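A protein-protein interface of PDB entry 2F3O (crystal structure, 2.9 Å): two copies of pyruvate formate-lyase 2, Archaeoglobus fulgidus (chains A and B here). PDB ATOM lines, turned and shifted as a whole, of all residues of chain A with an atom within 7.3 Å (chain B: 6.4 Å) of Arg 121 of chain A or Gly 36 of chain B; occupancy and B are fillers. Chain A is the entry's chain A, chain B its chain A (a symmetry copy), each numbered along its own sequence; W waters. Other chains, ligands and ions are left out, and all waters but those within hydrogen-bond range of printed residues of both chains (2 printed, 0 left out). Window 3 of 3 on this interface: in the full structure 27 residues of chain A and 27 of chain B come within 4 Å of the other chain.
OG1 of Thr 123 of chain A is in hydrogen-bond range of N of Ala 126 of chain A, 3.1 Å away.
The guanidinium group (NE) of Arg 121 of chain A lies within salt-bridge range of the side-chain carboxylate (OE2) of Glu 35 of chain B, 3.4 Å away.
The backbone NH (N) of Phe 127 of chain A lies within hydrogen-bond range of the backbone carbonyl oxygen (O) of Gly 36 of chain B, 3.0 Å away.
O of Lys 32 of chain B lies within hydrogen-bond range of NH1 of Arg 121 of chain A (3.2 Å).
The backbone carbonyl oxygen (O) of Gly 36 of chain B lies close to the backbone carbonyl oxygen (O) of Ala 126 of chain A.
No position is printed for both chains.
Of the 9 pairs that touch across the chains among the printed residues, none has its exchanged pair printed and touching as well.
Water W1 bridges O of Thr 123 of chain A (2.7 Å) and O of Gly 36 of chain B (2.9 Å).
Water W2 lies within hydrogen-bond range of the side-chain carboxylate (OE2) of Glu 35 of chain B (2.7 Å), the side-chain amino group (NZ) of Lys 122 of chain A (2.9 Å) and the backbone carbonyl oxygen (O) of Arg 121 of chain A (3.4 Å).
Of the 17 printed residues of chain A, 4 touch a printed residue of chain B.
Of the 9 printed residues of chain B, 5 touch a printed residue of chain A.
Hydrophobic or aromatic side chains of chain B that line the printed part of chain A: Pro 38.
Among the printed residues, Asp or Glu carboxylates within 4 Å of a Lys or Arg side-chain nitrogen of the other chain: Arg 121 of chain A with Glu 35 of chain B.
Among the printed residues, pairs that only touch across the chains: Arg 121 of chain A with Gly 36 of chain B, Ala 126 of chain A with Glu 37 of chain B, Phe 127 of chain A with Pro 38 of chain B, Pro 130 of chain A with Glu 37 of chain B and Pro 130 of chain A with Pro 38 of chain B.
Of the printed residues of chain B, Arg 121 of chain A touches Lys 32 (3.2 Å), Glu 35 (3.4 Å) and Gly 36 (3.3 Å).
Gly 36 of chain B touches three residues of chain A.
Printed residues of chain B within 4 Å of Ala 126 of chain A: Gly 36 (3.1 Å) and Glu 37 (3.99 Å).
Of the printed residues of chain A, Glu 37 of chain B touches Ala 126 and Pro 130.
Of the printed residues of chain B, Pro 130 of chain A touches Glu 37 and Pro 38.
Tyr 118 of chain A touches none of the printed residues of chain B.
Ala 116 of chain A touches none of the printed residues of chain B.
The nearest residue of chain A that does not touch Gly 36 of chain B is Thr 123 of chain A (4.7 Å).
The nearest printed residue of chain B that does not touch Ala 126 of chain A is Pro 38 of chain B (4.9 Å).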
ATOM      1  N   LEU A  84      10.029  -2.151 -18.226  1.00  0.00           N
ATOM      2  CA  LEU A  84       8.995  -3.040 -18.743  1.00  0.00           C
ATOM      3  C   LEU A  84       7.955  -3.365 -17.673  1.00  0.00           C
ATOM      4  O   LEU A  84       6.882  -3.892 -17.999  1.00  0.00           O
ATOM      5  CB  LEU A  84       9.561  -4.347 -19.310  1.00  0.00           C
ATOM      6  CG  LEU A  84      10.400  -4.444 -20.591  1.00  0.00           C
ATOM      7  CD1 LEU A  84      10.125  -5.770 -21.307  1.00  0.00           C
ATOM      8  CD2 LEU A  84      10.182  -3.278 -21.541  1.00  0.00           C
ATOM      9  N   ALA A 116       8.489  -3.259 -25.689  1.00  0.00           N
ATOM     10  CA  ALA A 116       8.351  -4.484 -24.882  1.00  0.00           C
ATOM     11  C   ALA A 116       8.693  -5.852 -25.520  1.00  0.00           C
ATOM     12  O   ALA A 116       9.183  -6.728 -24.805  1.00  0.00           O
ATOM     13  CB  ALA A 116       6.979  -4.548 -24.227  1.00  0.00           C
ATOM     14  N   PRO A 117       8.424  -6.066 -26.835  1.00  0.00           N
ATOM     15  CA  PRO A 117       8.957  -7.347 -27.304  1.00  0.00           C
ATOM     16  C   PRO A 117      10.469  -7.351 -27.575  1.00  0.00           C
ATOM     17  O   PRO A 117      11.072  -8.416 -27.524  1.00  0.00           O
ATOM     18  CB  PRO A 117       8.166  -7.627 -28.603  1.00  0.00           C
ATOM     19  CG  PRO A 117       7.156  -6.532 -28.723  1.00  0.00           C
ATOM     20  CD  PRO A 117       7.683  -5.384 -27.911  1.00  0.00           C
ATOM     21  N   TYR A 118      11.078  -6.196 -27.846  1.00  0.00           N
ATOM     22  CA  TYR A 118      12.529  -6.143 -28.065  1.00  0.00           C
ATOM     23  C   TYR A 118      13.310  -6.349 -26.763  1.00  0.00           C
ATOM     24  O   TYR A 118      14.200  -7.190 -26.684  1.00  0.00           O
ATOM     25  CB  TYR A 118      12.947  -4.820 -28.724  1.00  0.00           C
ATOM     26  CG  TYR A 118      14.429  -4.723 -29.036  1.00  0.00           C
ATOM     27  CD1 TYR A 118      14.965  -5.365 -30.141  1.00  0.00           C
ATOM     28  CD2 TYR A 118      15.290  -3.983 -28.232  1.00  0.00           C
ATOM     29  CE1 TYR A 118      16.311  -5.285 -30.437  1.00  0.00           C
ATOM     30  CE2 TYR A 118      16.640  -3.897 -28.520  1.00  0.00           C
ATOM     31  CZ  TYR A 118      17.148  -4.551 -29.626  1.00  0.00           C
ATOM     32  OH  TYR A 118      18.500  -4.489 -29.910  1.00  0.00           O
ATOM     33  N   TRP A 119      12.957  -5.583 -25.741  1.00  0.00           N
ATOM     34  CA  TRP A 119      13.702  -5.592 -24.498  1.00  0.00           C
ATOM     35  C   TRP A 119      13.422  -6.781 -23.593  1.00  0.00           C
ATOM     36  O   TRP A 119      14.190  -7.062 -22.689  1.00  0.00           O
ATOM     37  CB  TRP A 119      13.506  -4.273 -23.772  1.00  0.00           C
ATOM     38  CG  TRP A 119      14.272  -3.225 -24.445  1.00  0.00           C
ATOM     39  CD1 TRP A 119      13.791  -2.261 -25.272  1.00  0.00           C
ATOM     40  CD2 TRP A 119      15.691  -3.056 -24.404  1.00  0.00           C
ATOM     41  NE1 TRP A 119      14.820  -1.483 -25.734  1.00  0.00           N
ATOM     42  CE2 TRP A 119      15.999  -1.953 -25.216  1.00  0.00           C
ATOM     43  CE3 TRP A 119      16.731  -3.717 -23.738  1.00  0.00           C
ATOM     44  CZ2 TRP A 119      17.303  -1.502 -25.391  1.00  0.00           C
ATOM     45  CZ3 TRP A 119      18.021  -3.271 -23.914  1.00  0.00           C
ATOM     46  CH2 TRP A 119      18.298  -2.174 -24.730  1.00  0.00           C
ATOM     47  N   GLN A 120      12.313  -7.463 -23.835  1.00  0.00           N
ATOM     48  CA  GLN A 120      12.060  -8.766 -23.254  1.00  0.00           C
ATOM     49  C   GLN A 120      13.318  -9.580 -23.405  1.00  0.00           C
ATOM     50  O   GLN A 120      13.837  -9.719 -24.528  1.00  0.00           O
ATOM     51  CB  GLN A 120      10.951  -9.458 -24.049  1.00  0.00           C
ATOM     52  CG  GLN A 120      10.277 -10.600 -23.330  1.00  0.00           C
ATOM     53  CD  GLN A 120       9.663 -10.159 -22.013  1.00  0.00           C
ATOM     54  OE1 GLN A 120       9.053  -9.078 -21.913  1.00  0.00           O
ATOM     55  NE2 GLN A 120       9.820 -10.992 -20.990  1.00  0.00           N
ATOM     56  N   ARG A 121      13.834 -10.081 -22.287  1.00  0.00           N
ATOM     57  CA  ARG A 121      15.090 -10.879 -22.272  1.00  0.00           C
ATOM     58  C   ARG A 121      16.390 -10.211 -22.863  1.00  0.00           C
ATOM     59  O   ARG A 121      17.315 -10.883 -23.329  1.00  0.00           O
ATOM     60  CB  ARG A 121      14.849 -12.351 -22.712  1.00  0.00           C
ATOM     61  CG  ARG A 121      14.840 -12.634 -24.192  1.00  0.00           C
ATOM     62  CD  ARG A 121      14.279 -13.991 -24.481  1.00  0.00           C
ATOM     63  NE  ARG A 121      14.060 -14.127 -25.918  1.00  0.00           N
ATOM     64  CZ  ARG A 121      13.755 -15.271 -26.524  1.00  0.00           C
ATOM     65  NH1 ARG A 121      13.633 -16.392 -25.808  1.00  0.00           N
ATOM     66  NH2 ARG A 121      13.572 -15.297 -27.846  1.00  0.00           N
ATOM     67  N   LYS A 122      16.450  -8.886 -22.801  1.00  0.00           N
ATOM     68  CA  LYS A 122      17.681  -8.148 -23.062  1.00  0.00           C
ATOM     69  C   LYS A 122      18.016  -7.280 -21.850  1.00  0.00           C
ATOM     70  O   LYS A 122      18.841  -6.366 -21.940  1.00  0.00           O
ATOM     71  CB  LYS A 122      17.520  -7.253 -24.278  1.00  0.00           C
ATOM     72  CG  LYS A 122      17.755  -7.939 -25.587  1.00  0.00           C
ATOM     73  CD  LYS A 122      17.760  -6.948 -26.748  1.00  0.00           C
ATOM     74  CE  LYS A 122      17.636  -7.700 -28.060  1.00  0.00           C
ATOM     75  NZ  LYS A 122      16.469  -8.656 -28.107  1.00  0.00           N
ATOM     76  N   THR A 123      17.368  -7.579 -20.725  1.00  0.00           N
ATOM     77  CA  THR A 123      17.465  -6.748 -19.537  1.00  0.00           C
ATOM     78  C   THR A 123      18.550  -7.234 -18.593  1.00  0.00           C
ATOM     79  O   THR A 123      19.066  -8.337 -18.757  1.00  0.00           O
ATOM     80  CB  THR A 123      16.152  -6.740 -18.706  1.00  0.00           C
ATOM     81  OG1 THR A 123      15.940  -8.030 -18.109  1.00  0.00           O
ATOM     82  CG2 THR A 123      14.954  -6.342 -19.535  1.00  0.00           C
ATOM     83  N   ILE A 124      18.848  -6.408 -17.588  1.00  0.00           N
ATOM     84  CA  ILE A 124      19.754  -6.762 -16.506  1.00  0.00           C
ATOM     85  C   ILE A 124      19.259  -8.016 -15.811  1.00  0.00           C
ATOM     86  O   ILE A 124      20.031  -8.939 -15.590  1.00  0.00           O
ATOM     87  CB  ILE A 124      19.910  -5.594 -15.501  1.00  0.00           C
ATOM     88  CG1 ILE A 124      20.472  -4.375 -16.219  1.00  0.00           C
ATOM     89  CG2 ILE A 124      20.803  -5.970 -14.328  1.00  0.00           C
ATOM     90  CD1 ILE A 124      20.684  -3.188 -15.363  1.00  0.00           C
ATOM     91  N   GLU A 125      17.960  -8.071 -15.527  1.00  0.00           N
ATOM     92  CA  GLU A 125      17.354  -9.226 -14.857  1.00  0.00           C
ATOM     93  C   GLU A 125      17.478 -10.547 -15.646  1.00  0.00           C
ATOM     94  O   GLU A 125      17.672 -11.617 -15.054  1.00  0.00           O
ATOM     95  CB  GLU A 125      15.908  -8.904 -14.485  1.00  0.00           C
ATOM     96  CG  GLU A 125      14.911 -10.045 -14.606  1.00  0.00           C
ATOM     97  CD  GLU A 125      13.765  -9.888 -13.621  1.00  0.00           C
ATOM     98  OE1 GLU A 125      13.750  -8.840 -12.931  1.00  0.00           O
ATOM     99  OE2 GLU A 125      12.914 -10.811 -13.507  1.00  0.00           O
ATOM    100  N   ALA A 126      17.416 -10.457 -16.974  1.00  0.00           N
ATOM    101  CA  ALA A 126      17.622 -11.612 -17.839  1.00  0.00           C
ATOM    102  C   ALA A 126      19.023 -12.237 -17.713  1.00  0.00           C
ATOM    103  O   ALA A 126      19.161 -13.456 -17.779  1.00  0.00           O
ATOM    104  CB  ALA A 126      17.337 -11.247 -19.270  1.00  0.00           C
ATOM    105  N   PHE A 127      20.048 -11.403 -17.533  1.00  0.00           N
ATOM    106  CA  PHE A 127      21.412 -11.863 -17.235  1.00  0.00           C
ATOM    107  C   PHE A 127      21.483 -12.532 -15.891  1.00  0.00           C
ATOM    108  O   PHE A 127      22.034 -13.604 -15.766  1.00  0.00           O
ATOM    109  CB  PHE A 127      22.414 -10.697 -17.264  1.00  0.00           C
ATOM    110  CG  PHE A 127      23.867 -11.128 -17.256  1.00  0.00           C
ATOM    111  CD1 PHE A 127      24.592 -11.157 -18.430  1.00  0.00           C
ATOM    112  CD2 PHE A 127      24.507 -11.498 -16.073  1.00  0.00           C
ATOM    113  CE1 PHE A 127      25.914 -11.531 -18.426  1.00  0.00           C
ATOM    114  CE2 PHE A 127      25.823 -11.889 -16.061  1.00  0.00           C
ATOM    115  CZ  PHE A 127      26.532 -11.903 -17.238  1.00  0.00           C
ATOM    116  N   ALA A 128      20.944 -11.889 -14.876  1.00  0.00           N
ATOM    117  CA  ALA A 128      21.071 -12.414 -13.537  1.00  0.00           C
ATOM    118  C   ALA A 128      20.220 -13.634 -13.225  1.00  0.00           C
ATOM    119  O   ALA A 128      20.603 -14.424 -12.384  1.00  0.00           O
ATOM    120  CB  ALA A 128      20.785 -11.365 -12.574  1.00  0.00           C
ATOM    121  N   PHE A 129      19.075 -13.787 -13.881  1.00  0.00           N
ATOM    122  CA  PHE A 129      18.163 -14.892 -13.536  1.00  0.00           C
ATOM    123  C   PHE A 129      18.761 -16.309 -13.480  1.00  0.00           C
ATOM    124  O   PHE A 129      18.596 -16.982 -12.457  1.00  0.00           O
ATOM    125  CB  PHE A 129      16.868 -14.890 -14.363  1.00  0.00           C
ATOM    126  CG  PHE A 129      15.828 -15.839 -13.831  1.00  0.00           C
ATOM    127  CD1 PHE A 129      14.910 -15.404 -12.865  1.00  0.00           C
ATOM    128  CD2 PHE A 129      15.770 -17.168 -14.275  1.00  0.00           C
ATOM    129  CE1 PHE A 129      13.946 -16.269 -12.338  1.00  0.00           C
ATOM    130  CE2 PHE A 129      14.814 -18.050 -13.761  1.00  0.00           C
ATOM    131  CZ  PHE A 129      13.892 -17.596 -12.785  1.00  0.00           C
ATOM    132  N   PRO A 130      19.473 -16.765 -14.550  1.00  0.00           N
ATOM    133  CA  PRO A 130      19.888 -18.165 -14.458  1.00  0.00           C
ATOM    134  C   PRO A 130      20.912 -18.390 -13.349  1.00  0.00           C
ATOM    135  O   PRO A 130      21.126 -19.524 -12.945  1.00  0.00           O
ATOM    136  CB  PRO A 130      20.509 -18.425 -15.829  1.00  0.00           C
ATOM    137  CG  PRO A 130      20.930 -17.131 -16.287  1.00  0.00           C
ATOM    138  CD  PRO A 130      19.938 -16.165 -15.819  1.00  0.00           C
ATOM    139  N   VAL A 508      25.759  -5.942 -19.032  1.00  0.00           N
ATOM    140  CA  VAL A 508      24.719  -5.539 -20.001  1.00  0.00           C
ATOM    141  C   VAL A 508      24.345  -4.062 -19.969  1.00  0.00           C
ATOM    142  O   VAL A 508      23.611  -3.580 -20.827  1.00  0.00           O
ATOM    143  CB  VAL A 508      23.426  -6.403 -19.906  1.00  0.00           C
ATOM    144  CG1 VAL A 508      23.741  -7.822 -19.460  1.00  0.00           C
ATOM    145  CG2 VAL A 508      22.411  -5.770 -18.976  1.00  0.00           C
ATOM    146  N   MET B  31      20.532 -21.222 -28.630  1.00  0.00           N
ATOM    147  CA  MET B  31      20.870 -19.801 -28.525  1.00  0.00           C
ATOM    148  C   MET B  31      19.641 -18.890 -28.556  1.00  0.00           C
ATOM    149  O   MET B  31      19.642 -17.826 -27.946  1.00  0.00           O
ATOM    150  CB  MET B  31      21.882 -19.379 -29.600  1.00  0.00           C
ATOM    151  CG  MET B  31      23.286 -19.958 -29.433  1.00  0.00           C
ATOM    152  SD  MET B  31      24.229 -19.423 -27.987  1.00  0.00           S
ATOM    153  CE  MET B  31      24.895 -17.896 -28.584  1.00  0.00           C
ATOM    154  N   LYS B  32      18.589 -19.304 -29.246  1.00  0.00           N
ATOM    155  CA  LYS B  32      17.349 -18.574 -29.180  1.00  0.00           C
ATOM    156  C   LYS B  32      16.674 -18.766 -27.822  1.00  0.00           C
ATOM    157  O   LYS B  32      16.153 -17.805 -27.262  1.00  0.00           O
ATOM    158  CB  LYS B  32      16.423 -18.998 -30.308  1.00  0.00           C
ATOM    159  CG  LYS B  32      16.521 -18.121 -31.531  1.00  0.00           C
ATOM    160  CD  LYS B  32      16.081 -18.846 -32.797  1.00  0.00           C
ATOM    161  CE  LYS B  32      15.709 -17.841 -33.869  1.00  0.00           C
ATOM    162  NZ  LYS B  32      15.563 -18.510 -35.182  1.00  0.00           N
ATOM    163  N   GLN B  33      16.705 -19.985 -27.272  1.00  0.00           N
ATOM    164  CA  GLN B  33      16.132 -20.218 -25.939  1.00  0.00           C
ATOM    165  C   GLN B  33      16.911 -19.474 -24.862  1.00  0.00           C
ATOM    166  O   GLN B  33      16.400 -19.283 -23.751  1.00  0.00           O
ATOM    167  CB  GLN B  33      16.116 -21.706 -25.521  1.00  0.00           C
ATOM    168  CG  GLN B  33      15.269 -22.690 -26.349  1.00  0.00           C
ATOM    169  CD  GLN B  33      13.837 -22.217 -26.594  1.00  0.00           C
ATOM    170  OE1 GLN B  33      13.107 -21.849 -25.656  1.00  0.00           O
ATOM    171  NE2 GLN B  33      13.426 -22.228 -27.870  1.00  0.00           N
ATOM    172  N   THR B  34      18.149 -19.078 -25.153  1.00  0.00           N
ATOM    173  CA  THR B  34      18.987 -18.564 -24.076  1.00  0.00           C
ATOM    174  C   THR B  34      19.318 -17.078 -24.101  1.00  0.00           C
ATOM    175  O   THR B  34      20.037 -16.626 -23.228  1.00  0.00           O
ATOM    176  CB  THR B  34      20.295 -19.362 -23.888  1.00  0.00           C
ATOM    177  OG1 THR B  34      21.058 -19.323 -25.092  1.00  0.00           O
ATOM    178  CG2 THR B  34      20.011 -20.786 -23.488  1.00  0.00           C
ATOM    179  N   GLU B  35      18.785 -16.321 -25.051  1.00  0.00           N
ATOM    180  CA  GLU B  35      19.163 -14.908 -25.187  1.00  0.00           C
ATOM    181  C   GLU B  35      19.092 -14.101 -23.888  1.00  0.00           C
ATOM    182  O   GLU B  35      18.189 -14.282 -23.080  1.00  0.00           O
ATOM    183  CB  GLU B  35      18.307 -14.217 -26.239  1.00  0.00           C
ATOM    184  CG  GLU B  35      18.535 -14.691 -27.649  1.00  0.00           C
ATOM    185  CD  GLU B  35      17.412 -14.267 -28.570  1.00  0.00           C
ATOM    186  OE1 GLU B  35      17.372 -14.751 -29.718  1.00  0.00           O
ATOM    187  OE2 GLU B  35      16.563 -13.452 -28.144  1.00  0.00           O
ATOM    188  N   GLY B  36      20.073 -13.227 -23.681  1.00  0.00           N
ATOM    189  CA  GLY B  36      20.121 -12.412 -22.479  1.00  0.00           C
ATOM    190  C   GLY B  36      20.724 -13.086 -21.258  1.00  0.00           C
ATOM    191  O   GLY B  36      20.857 -12.456 -20.220  1.00  0.00           O
ATOM    192  N   GLU B  37      21.078 -14.366 -21.369  1.00  0.00           N
ATOM    193  CA  GLU B  37      21.798 -15.065 -20.310  1.00  0.00           C
ATOM    194  C   GLU B  37      23.296 -14.792 -20.476  1.00  0.00           C
ATOM    195  O   GLU B  37      23.710 -14.343 -21.553  1.00  0.00           O
ATOM    196  CB  GLU B  37      21.478 -16.562 -20.361  1.00  0.00           C
ATOM    197  CG  GLU B  37      20.113 -16.887 -19.830  1.00  0.00           C
ATOM    198  CD  GLU B  37      19.775 -18.345 -19.918  1.00  0.00           C
ATOM    199  OE1 GLU B  37      20.658 -19.191 -19.688  1.00  0.00           O
ATOM    200  OE2 GLU B  37      18.608 -18.641 -20.224  1.00  0.00           O
ATOM    201  N   PRO B  38      24.099 -15.013 -19.400  1.00  0.00           N
ATOM    202  CA  PRO B  38      25.551 -14.905 -19.455  1.00  0.00           C
ATOM    203  C   PRO B  38      26.118 -15.741 -20.585  1.00  0.00           C
ATOM    204  O   PRO B  38      25.877 -16.940 -20.608  1.00  0.00           O
ATOM    205  CB  PRO B  38      25.980 -15.507 -18.117  1.00  0.00           C
ATOM    206  CG  PRO B  38      24.864 -15.289 -17.223  1.00  0.00           C
ATOM    207  CD  PRO B  38      23.647 -15.362 -18.039  1.00  0.00           C
ATOM    208  N   ARG B  42      25.425 -19.567 -22.019  1.00  0.00           N
ATOM    209  CA  ARG B  42      24.774 -19.785 -23.312  1.00  0.00           C
ATOM    210  C   ARG B  42      25.549 -20.754 -24.177  1.00  0.00           C
ATOM    211  O   ARG B  42      24.952 -21.629 -24.797  1.00  0.00           O
ATOM    212  CB  ARG B  42      24.540 -18.480 -24.072  1.00  0.00           C
ATOM    213  CG  ARG B  42      23.845 -17.458 -23.228  1.00  0.00           C
ATOM    214  CD  ARG B  42      22.850 -16.628 -23.974  1.00  0.00           C
ATOM    215  NE  ARG B  42      23.360 -15.882 -25.111  1.00  0.00           N
ATOM    216  CZ  ARG B  42      22.861 -15.973 -26.337  1.00  0.00           C
ATOM    217  NH1 ARG B  42      21.842 -16.788 -26.571  1.00  0.00           N
ATOM    218  NH2 ARG B  42      23.375 -15.249 -27.328  1.00  0.00           N
HETATM  219  O   HOH W   1      20.503  -9.640 -20.626  1.00  0.00           O
HETATM  220  O   HOH W   2      17.136 -11.163 -26.746  1.00  0.00           O
